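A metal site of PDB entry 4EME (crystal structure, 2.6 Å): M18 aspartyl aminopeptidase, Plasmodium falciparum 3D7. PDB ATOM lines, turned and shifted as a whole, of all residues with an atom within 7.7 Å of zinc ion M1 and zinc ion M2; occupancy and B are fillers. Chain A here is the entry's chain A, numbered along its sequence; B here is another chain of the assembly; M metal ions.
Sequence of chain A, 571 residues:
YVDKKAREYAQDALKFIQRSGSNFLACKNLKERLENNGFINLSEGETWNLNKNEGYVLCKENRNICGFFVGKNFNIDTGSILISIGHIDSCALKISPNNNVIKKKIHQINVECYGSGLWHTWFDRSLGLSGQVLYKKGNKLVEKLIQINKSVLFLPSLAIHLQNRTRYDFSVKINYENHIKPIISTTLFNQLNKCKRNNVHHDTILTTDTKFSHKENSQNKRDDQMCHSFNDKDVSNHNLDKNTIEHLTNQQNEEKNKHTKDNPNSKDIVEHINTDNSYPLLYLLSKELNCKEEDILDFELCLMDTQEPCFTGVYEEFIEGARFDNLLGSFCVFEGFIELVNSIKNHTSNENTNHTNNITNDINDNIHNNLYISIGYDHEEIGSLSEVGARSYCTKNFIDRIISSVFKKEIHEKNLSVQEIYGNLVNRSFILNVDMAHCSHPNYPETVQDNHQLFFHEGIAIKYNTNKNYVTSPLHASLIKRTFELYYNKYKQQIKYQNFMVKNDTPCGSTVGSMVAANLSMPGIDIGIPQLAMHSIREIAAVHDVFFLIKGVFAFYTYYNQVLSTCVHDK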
ATOM      1  N   GLY A  86      30.610 -18.290 -15.746  1.00  0.00           N
ATOM      2  CA  GLY A  86      29.435 -19.126 -15.601  1.00  0.00           C
ATOM      3  C   GLY A  86      29.283 -19.885 -16.897  1.00  0.00           C
ATOM      4  O   GLY A  86      30.132 -19.771 -17.792  1.00  0.00           O
ATOM      5  N   HIS A  87      28.223 -20.676 -17.032  1.00  0.00           N
ATOM      6  CA  HIS A  87      27.988 -21.368 -18.281  1.00  0.00           C
ATOM      7  C   HIS A  87      26.538 -21.269 -18.575  1.00  0.00           C
ATOM      8  O   HIS A  87      25.735 -21.373 -17.661  1.00  0.00           O
ATOM      9  CB  HIS A  87      28.556 -22.799 -18.311  1.00  0.00           C
ATOM     10  CG  HIS A  87      27.846 -23.795 -17.451  1.00  0.00           C
ATOM     11  ND1 HIS A  87      26.739 -24.490 -17.912  1.00  0.00           N
ATOM     12  CD2 HIS A  87      28.167 -24.250 -16.215  1.00  0.00           C
ATOM     13  CE1 HIS A  87      26.391 -25.307 -16.937  1.00  0.00           C
ATOM     14  NE2 HIS A  87      27.223 -25.206 -15.894  1.00  0.00           N
ATOM     15  N   ASP A  89      24.650 -23.043 -20.978  1.00  0.00           N
ATOM     16  CA  ASP A  89      23.997 -24.279 -21.460  1.00  0.00           C
ATOM     17  C   ASP A  89      23.567 -25.107 -20.249  1.00  0.00           C
ATOM     18  O   ASP A  89      24.193 -25.048 -19.190  1.00  0.00           O
ATOM     19  CB  ASP A  89      24.982 -25.114 -22.293  1.00  0.00           C
ATOM     20  CG  ASP A  89      26.168 -25.661 -21.494  1.00  0.00           C
ATOM     21  OD1 ASP A  89      26.779 -24.885 -20.725  1.00  0.00           O
ATOM     22  OD2 ASP A  89      26.476 -26.873 -21.638  1.00  0.00           O
ATOM     23  N   SER A  90      22.525 -25.908 -20.406  1.00  0.00           N
ATOM     24  CA  SER A  90      22.069 -26.813 -19.358  1.00  0.00           C
ATOM     25  C   SER A  90      21.726 -28.110 -20.044  1.00  0.00           C
ATOM     26  O   SER A  90      21.657 -28.165 -21.274  1.00  0.00           O
ATOM     27  CB  SER A  90      20.811 -26.272 -18.680  1.00  0.00           C
ATOM     28  OG  SER A  90      21.055 -25.016 -18.078  1.00  0.00           O
ATOM     29  N   CYS A  91      21.467 -29.156 -19.255  1.00  0.00           N
ATOM     30  CA  CYS A  91      21.017 -30.448 -19.746  1.00  0.00           C
ATOM     31  C   CYS A  91      19.697 -30.240 -20.417  1.00  0.00           C
ATOM     32  O   CYS A  91      18.833 -29.523 -19.902  1.00  0.00           O
ATOM     33  CB  CYS A  91      20.903 -31.434 -18.588  1.00  0.00           C
ATOM     34  SG  CYS A  91      22.514 -31.927 -17.926  1.00  0.00           S
ATOM     35  N   GLY A 115      23.843 -33.339 -22.395  1.00  0.00           N
ATOM     36  CA  GLY A 115      24.310 -33.295 -21.005  1.00  0.00           C
ATOM     37  C   GLY A 115      23.828 -34.517 -20.227  1.00  0.00           C
ATOM     38  O   GLY A 115      23.001 -35.292 -20.724  1.00  0.00           O
ATOM     39  N   SER A 116      24.385 -34.732 -19.027  1.00  0.00           N
ATOM     40  CA  SER A 116      24.022 -35.889 -18.211  1.00  0.00           C
ATOM     41  C   SER A 116      22.804 -35.581 -17.321  1.00  0.00           C
ATOM     42  O   SER A 116      22.898 -35.429 -16.089  1.00  0.00           O
ATOM     43  CB  SER A 116      25.228 -36.409 -17.436  1.00  0.00           C
ATOM     44  OG  SER A 116      25.638 -35.421 -16.504  1.00  0.00           O
ATOM     45  N   PHE A 324      18.701 -23.923 -13.150  1.00  0.00           N
ATOM     46  CA  PHE A 324      19.437 -23.207 -12.073  1.00  0.00           C
ATOM     47  C   PHE A 324      20.921 -23.430 -12.282  1.00  0.00           C
ATOM     48  O   PHE A 324      21.705 -22.494 -12.193  1.00  0.00           O
ATOM     49  CB  PHE A 324      18.998 -23.640 -10.661  1.00  0.00           C
ATOM     50  CG  PHE A 324      17.704 -22.997 -10.192  1.00  0.00           C
ATOM     51  CD1 PHE A 324      16.910 -22.250 -11.072  1.00  0.00           C
ATOM     52  CD2 PHE A 324      17.261 -23.152  -8.883  1.00  0.00           C
ATOM     53  CE1 PHE A 324      15.723 -21.667 -10.648  1.00  0.00           C
ATOM     54  CE2 PHE A 324      16.062 -22.572  -8.467  1.00  0.00           C
ATOM     55  CZ  PHE A 324      15.310 -21.825  -9.344  1.00  0.00           C
ATOM     56  N   ASP A 325      21.264 -24.673 -12.672  1.00  0.00           N
ATOM     57  CA  ASP A 325      22.580 -25.076 -13.125  1.00  0.00           C
ATOM     58  C   ASP A 325      22.560 -24.860 -14.663  1.00  0.00           C
ATOM     59  O   ASP A 325      21.942 -25.651 -15.371  1.00  0.00           O
ATOM     60  CB  ASP A 325      22.881 -26.531 -12.768  1.00  0.00           C
ATOM     61  CG  ASP A 325      24.147 -27.022 -13.446  1.00  0.00           C
ATOM     62  OD1 ASP A 325      25.077 -26.217 -13.611  1.00  0.00           O
ATOM     63  OD2 ASP A 325      24.192 -28.205 -13.832  1.00  0.00           O
ATOM     64  N   ASN A 326      23.180 -23.777 -15.180  1.00  0.00           N
ATOM     65  CA  ASN A 326      23.921 -22.759 -14.409  1.00  0.00           C
ATOM     66  C   ASN A 326      23.480 -21.342 -14.745  1.00  0.00           C
ATOM     67  O   ASN A 326      24.274 -20.406 -14.720  1.00  0.00           O
ATOM     68  CB  ASN A 326      25.441 -22.942 -14.531  1.00  0.00           C
ATOM     69  CG  ASN A 326      26.261 -22.111 -13.589  1.00  0.00           C
ATOM     70  OD1 ASN A 326      25.859 -21.833 -12.450  1.00  0.00           O
ATOM     71  ND2 ASN A 326      27.422 -21.649 -14.055  1.00  0.00           N
ATOM     72  N   LEU A 327      22.182 -21.176 -15.034  1.00  0.00           N
ATOM     73  CA  LEU A 327      21.614 -19.871 -15.337  1.00  0.00           C
ATOM     74  C   LEU A 327      21.420 -19.044 -14.068  1.00  0.00           C
ATOM     75  O   LEU A 327      21.398 -17.811 -14.153  1.00  0.00           O
ATOM     76  CB  LEU A 327      20.330 -19.981 -16.181  1.00  0.00           C
ATOM     77  CG  LEU A 327      20.494 -20.544 -17.600  1.00  0.00           C
ATOM     78  CD1 LEU A 327      19.285 -20.268 -18.418  1.00  0.00           C
ATOM     79  CD2 LEU A 327      21.703 -19.930 -18.305  1.00  0.00           C
ATOM     80  N   GLU A 380      29.492 -26.495 -21.459  1.00  0.00           N
ATOM     81  CA  GLU A 380      30.017 -27.062 -20.219  1.00  0.00           C
ATOM     82  C   GLU A 380      29.456 -28.461 -19.981  1.00  0.00           C
ATOM     83  O   GLU A 380      30.220 -29.366 -19.628  1.00  0.00           O
ATOM     84  CB  GLU A 380      29.697 -26.171 -19.013  1.00  0.00           C
ATOM     85  CG  GLU A 380      30.487 -26.502 -17.750  1.00  0.00           C
ATOM     86  CD  GLU A 380      29.973 -27.574 -16.809  1.00  0.00           C
ATOM     87  OE1 GLU A 380      28.758 -27.877 -16.847  1.00  0.00           O
ATOM     88  OE2 GLU A 380      30.775 -28.063 -15.984  1.00  0.00           O
ATOM     89  N   GLU A 381      28.144 -28.657 -20.217  1.00  0.00           N
ATOM     90  CA  GLU A 381      27.475 -29.944 -20.006  1.00  0.00           C
ATOM     91  C   GLU A 381      28.023 -31.131 -20.804  1.00  0.00           C
ATOM     92  O   GLU A 381      27.859 -32.279 -20.374  1.00  0.00           O
ATOM     93  CB  GLU A 381      25.937 -29.818 -20.101  1.00  0.00           C
ATOM     94  CG  GLU A 381      25.324 -28.892 -19.059  1.00  0.00           C
ATOM     95  CD  GLU A 381      25.486 -29.188 -17.574  1.00  0.00           C
ATOM     96  OE1 GLU A 381      26.155 -30.183 -17.211  1.00  0.00           O
ATOM     97  OE2 GLU A 381      24.940 -28.407 -16.771  1.00  0.00           O
ATOM     98  N   VAL A 434      32.173 -19.679 -11.287  1.00  0.00           N
ATOM     99  CA  VAL A 434      30.870 -19.819 -10.625  1.00  0.00           C
ATOM    100  C   VAL A 434      30.002 -20.893 -11.291  1.00  0.00           C
ATOM    101  O   VAL A 434      29.665 -20.805 -12.482  1.00  0.00           O
ATOM    102  CB  VAL A 434      30.135 -18.467 -10.539  1.00  0.00           C
ATOM    103  CG1 VAL A 434      28.762 -18.624  -9.849  1.00  0.00           C
ATOM    104  CG2 VAL A 434      30.993 -17.391  -9.859  1.00  0.00           C
ATOM    105  N   ASP A 435      29.648 -21.905 -10.503  1.00  0.00           N
ATOM    106  CA  ASP A 435      28.797 -23.010 -10.929  1.00  0.00           C
ATOM    107  C   ASP A 435      28.128 -23.557  -9.706  1.00  0.00           C
ATOM    108  O   ASP A 435      28.710 -23.531  -8.626  1.00  0.00           O
ATOM    109  CB  ASP A 435      29.616 -24.122 -11.619  1.00  0.00           C
ATOM    110  CG  ASP A 435      28.853 -24.945 -12.642  1.00  0.00           C
ATOM    111  OD1 ASP A 435      27.591 -25.019 -12.541  1.00  0.00           O
ATOM    112  OD2 ASP A 435      29.500 -25.536 -13.525  1.00  0.00           O
ATOM    113  N   MET A 436      26.898 -24.054  -9.866  1.00  0.00           N
ATOM    114  CA  MET A 436      26.102 -24.574  -8.755  1.00  0.00           C
ATOM    115  C   MET A 436      26.765 -25.687  -7.952  1.00  0.00           C
ATOM    116  O   MET A 436      27.569 -26.452  -8.507  1.00  0.00           O
ATOM    117  CB  MET A 436      24.714 -24.989  -9.243  1.00  0.00           C
ATOM    118  CG  MET A 436      23.939 -23.858  -9.872  1.00  0.00           C
ATOM    119  SD  MET A 436      23.722 -22.448  -8.761  1.00  0.00           S
ATOM    120  CE  MET A 436      22.328 -23.041  -7.793  1.00  0.00           C
ATOM    121  N   ALA A 437      26.447 -25.758  -6.644  1.00  0.00           N
ATOM    122  CA  ALA A 437      26.985 -26.743  -5.701  1.00  0.00           C
ATOM    123  C   ALA A 437      25.877 -27.613  -5.092  1.00  0.00           C
ATOM    124  O   ALA A 437      24.693 -27.241  -5.142  1.00  0.00           O
ATOM    125  CB  ALA A 437      27.771 -26.062  -4.612  1.00  0.00           C
ATOM    126  N   LYS A 463      34.348 -24.556  -3.276  1.00  0.00           N
ATOM    127  CA  LYS A 463      34.481 -25.939  -3.707  1.00  0.00           C
ATOM    128  C   LYS A 463      35.910 -26.404  -3.898  1.00  0.00           C
ATOM    129  O   LYS A 463      36.605 -25.863  -4.740  1.00  0.00           O
ATOM    130  CB  LYS A 463      33.666 -26.148  -5.001  1.00  0.00           C
ATOM    131  CG  LYS A 463      32.175 -25.854  -4.840  1.00  0.00           C
ATOM    132  CD  LYS A 463      31.552 -25.207  -6.074  1.00  0.00           C
ATOM    133  CE  LYS A 463      31.424 -26.158  -7.232  1.00  0.00           C
ATOM    134  NZ  LYS A 463      30.393 -25.686  -8.189  1.00  0.00           N
ATOM    135  N   SER A 510      33.199 -32.148 -12.969  1.00  0.00           N
ATOM    136  CA  SER A 510      34.218 -31.129 -13.190  1.00  0.00           C
ATOM    137  C   SER A 510      33.574 -29.776 -13.569  1.00  0.00           C
ATOM    138  O   SER A 510      32.384 -29.723 -13.918  1.00  0.00           O
ATOM    139  CB  SER A 510      35.207 -31.577 -14.251  1.00  0.00           C
ATOM    140  OG  SER A 510      36.050 -32.611 -13.754  1.00  0.00           O
ATOM    141  N   THR A 511      34.370 -28.685 -13.479  1.00  0.00           N
ATOM    142  CA  THR A 511      33.972 -27.325 -13.835  1.00  0.00           C
ATOM    143  C   THR A 511      34.930 -26.798 -14.927  1.00  0.00           C
ATOM    144  O   THR A 511      35.941 -27.423 -15.218  1.00  0.00           O
ATOM    145  CB  THR A 511      33.982 -26.404 -12.603  1.00  0.00           C
ATOM    146  OG1 THR A 511      35.307 -26.339 -12.071  1.00  0.00           O
ATOM    147  CG2 THR A 511      32.988 -26.825 -11.526  1.00  0.00           C
ATOM    148  N   VAL A 512      34.617 -25.651 -15.502  1.00  0.00           N
ATOM    149  CA  VAL A 512      35.467 -25.038 -16.517  1.00  0.00           C
ATOM    150  C   VAL A 512      36.667 -24.285 -15.920  1.00  0.00           C
ATOM    151  O   VAL A 512      37.499 -23.801 -16.669  1.00  0.00           O
ATOM    152  CB  VAL A 512      34.661 -24.151 -17.477  1.00  0.00           C
ATOM    153  CG1 VAL A 512      33.660 -24.975 -18.258  1.00  0.00           C
ATOM    154  CG2 VAL A 512      33.973 -23.000 -16.758  1.00  0.00           C
ATOM    155  N   GLN A 531      22.350 -26.098  -4.052  1.00  0.00           N
ATOM    156  CA  GLN A 531      21.044 -26.464  -4.606  1.00  0.00           C
ATOM    157  C   GLN A 531      20.831 -27.961  -4.432  1.00  0.00           C
ATOM    158  O   GLN A 531      21.788 -28.688  -4.147  1.00  0.00           O
ATOM    159  CB  GLN A 531      20.928 -26.069  -6.095  1.00  0.00           C
ATOM    160  CG  GLN A 531      21.853 -26.863  -7.004  1.00  0.00           C
ATOM    161  CD  GLN A 531      21.303 -27.077  -8.382  1.00  0.00           C
ATOM    162  OE1 GLN A 531      21.826 -26.574  -9.355  1.00  0.00           O
ATOM    163  NE2 GLN A 531      20.281 -27.908  -8.499  1.00  0.00           N
ATOM    164  N   MET A 534      20.373 -31.436  -8.883  1.00  0.00           N
ATOM    165  CA  MET A 534      21.125 -30.953 -10.045  1.00  0.00           C
ATOM    166  C   MET A 534      20.967 -31.899 -11.211  1.00  0.00           C
ATOM    167  O   MET A 534      21.124 -33.109 -11.050  1.00  0.00           O
ATOM    168  CB  MET A 534      22.606 -30.728  -9.708  1.00  0.00           C
ATOM    169  CG  MET A 534      23.247 -29.627 -10.550  1.00  0.00           C
ATOM    170  SD  MET A 534      24.988 -29.295 -10.138  1.00  0.00           S
ATOM    171  CE  MET A 534      24.803 -28.606  -8.480  1.00  0.00           C
ATOM    172  N   HIS A 535      20.646 -31.324 -12.394  1.00  0.00           N
ATOM    173  CA  HIS A 535      20.422 -31.989 -13.688  1.00  0.00           C
ATOM    174  C   HIS A 535      18.977 -32.463 -13.937  1.00  0.00           C
ATOM    175  O   HIS A 535      18.687 -33.125 -14.934  1.00  0.00           O
ATOM    176  CB  HIS A 535      21.526 -33.006 -14.067  1.00  0.00           C
ATOM    177  CG  HIS A 535      22.832 -32.343 -14.371  1.00  0.00           C
ATOM    178  ND1 HIS A 535      23.805 -33.001 -15.100  1.00  0.00           N
ATOM    179  CD2 HIS A 535      23.251 -31.086 -14.095  1.00  0.00           C
ATOM    180  CE1 HIS A 535      24.798 -32.137 -15.209  1.00  0.00           C
ATOM    181  NE2 HIS A 535      24.502 -30.965 -14.633  1.00  0.00           N
ATOM    182  N   GLU A 539      15.036 -27.864 -10.479  1.00  0.00           N
ATOM    183  CA  GLU A 539      15.974 -27.851  -9.364  1.00  0.00           C
ATOM    184  C   GLU A 539      15.496 -26.872  -8.291  1.00  0.00           C
ATOM    185  O   GLU A 539      14.519 -26.171  -8.516  1.00  0.00           O
ATOM    186  CB  GLU A 539      17.364 -27.495  -9.909  1.00  0.00           C
ATOM    187  CG  GLU A 539      17.771 -28.350 -11.111  1.00  0.00           C
ATOM    188  CD  GLU A 539      18.971 -27.848 -11.898  1.00  0.00           C
ATOM    189  OE1 GLU A 539      19.210 -26.628 -11.925  1.00  0.00           O
ATOM    190  OE2 GLU A 539      19.681 -28.701 -12.493  1.00  0.00           O
ATOM    191  N   ILE B 160      22.508 -36.048 -10.068  1.00  0.00           N
ATOM    192  CA  ILE B 160      23.068 -37.170 -10.827  1.00  0.00           C
ATOM    193  C   ILE B 160      24.569 -37.392 -10.497  1.00  0.00           C
ATOM    194  O   ILE B 160      25.080 -38.511 -10.593  1.00  0.00           O
ATOM    195  CB  ILE B 160      22.815 -37.009 -12.359  1.00  0.00           C
ATOM    196  CG1 ILE B 160      23.053 -38.348 -13.128  1.00  0.00           C
ATOM    197  CG2 ILE B 160      23.590 -35.825 -12.944  1.00  0.00           C
ATOM    198  CD1 ILE B 160      22.408 -38.499 -14.452  1.00  0.00           C
ATOM    199  N   HIS B 161      25.241 -36.311 -10.087  1.00  0.00           N
ATOM    200  CA  HIS B 161      26.663 -36.279  -9.739  1.00  0.00           C
ATOM    201  C   HIS B 161      26.931 -37.147  -8.517  1.00  0.00           C
ATOM    202  O   HIS B 161      28.000 -37.745  -8.421  1.00  0.00           O
ATOM    203  CB  HIS B 161      27.095 -34.837  -9.470  1.00  0.00           C
ATOM    204  CG  HIS B 161      26.622 -33.852 -10.502  1.00  0.00           C
ATOM    205  ND1 HIS B 161      25.281 -33.538 -10.636  1.00  0.00           N
ATOM    206  CD2 HIS B 161      27.331 -33.126 -11.388  1.00  0.00           C
ATOM    207  CE1 HIS B 161      25.220 -32.650 -11.612  1.00  0.00           C
ATOM    208  NE2 HIS B 161      26.434 -32.365 -12.093  1.00  0.00           N
HETATM  209 ZN    ZN M   1      25.802 -29.228 -14.881  1.00  0.00          ZN
HETATM  210 ZN    ZN M   2      27.220 -26.479 -13.998  1.00  0.00          ZN
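The backbone carbonyl oxygen (O) of Asp 325 is in hydrogen-bond range of the side-chain hydroxyl (OG) of Ser 90, at 2.9 Å.
N of Asp 325 is in hydrogen-bond range of OE1 of Glu 539, at 2.9 Å.
The backbone NH (N) of His 535 lies within hydrogen-bond range of the side-chain carboxylate (OE2) of Glu 539.
The backbone NH (N) of Glu 381 sits at hydrogen-bond distance from the side-chain carboxylate (OD2) of Asp 89 (2.8 Å).
A ring nitrogen (NE2) of His 87 sits close to the side-chain carboxylate (OE1) of Glu 380 (3.2 Å).
N of His 87 sits close to ND2 of Asn 326, 3.2 Å away.
The side-chain carboxylate of Asp 89 sits at hydrogen-bond distance from the backbone NH of Glu 380, 3.0 Å away.
O of Val 434 sits at hydrogen-bond distance from ND2 of Asn 326, 2.9 Å away.
Glu 380 touches zinc ion M1 (OE1 to ZN, 3.8 Å).
Four residues have an atom within 4 Å of zinc ion M1: Asp 325, Glu 380, Glu 381 and His 535.
The nearest printed residue that does not touch zinc ion M1 is His 161 of chain B (4.2 Å).
Asn 326 touches zinc ion M2 (CB to ZN, 3.99 Å).
Glu 380 touches zinc ion M2.
Of the 27 residues printed, 5 come within 4 Å of zinc ion M2.
The nearest printed residue that does not touch zinc ion M2 is Glu 381 (4.1 Å).
Zinc ion M1 is bound by OD2 of Asp 325 (2.2 Å).
Zinc ion M1 is bound by NE2 of His 535 (2.2 Å).
Zinc ion M1 is bound by OE2 of Glu 381.
Zinc ion M1 is bound by OE1 of Glu 381 (2.5 Å).
Zinc ion M1 has four donor atoms within binding distance.
The side-chain carboxylate (OD1) of Asp 435 binds zinc ion M2 (2.1 Å).
The side-chain carboxylate (OD1) of Asp 325 binds zinc ion M2 (2.2 Å).
Zinc ion M2 is bound by a ring nitrogen (NE2) of His 87, 2.3 Å away.
OD2 of Asp 435 binds zinc ion M2 (2.5 Å).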
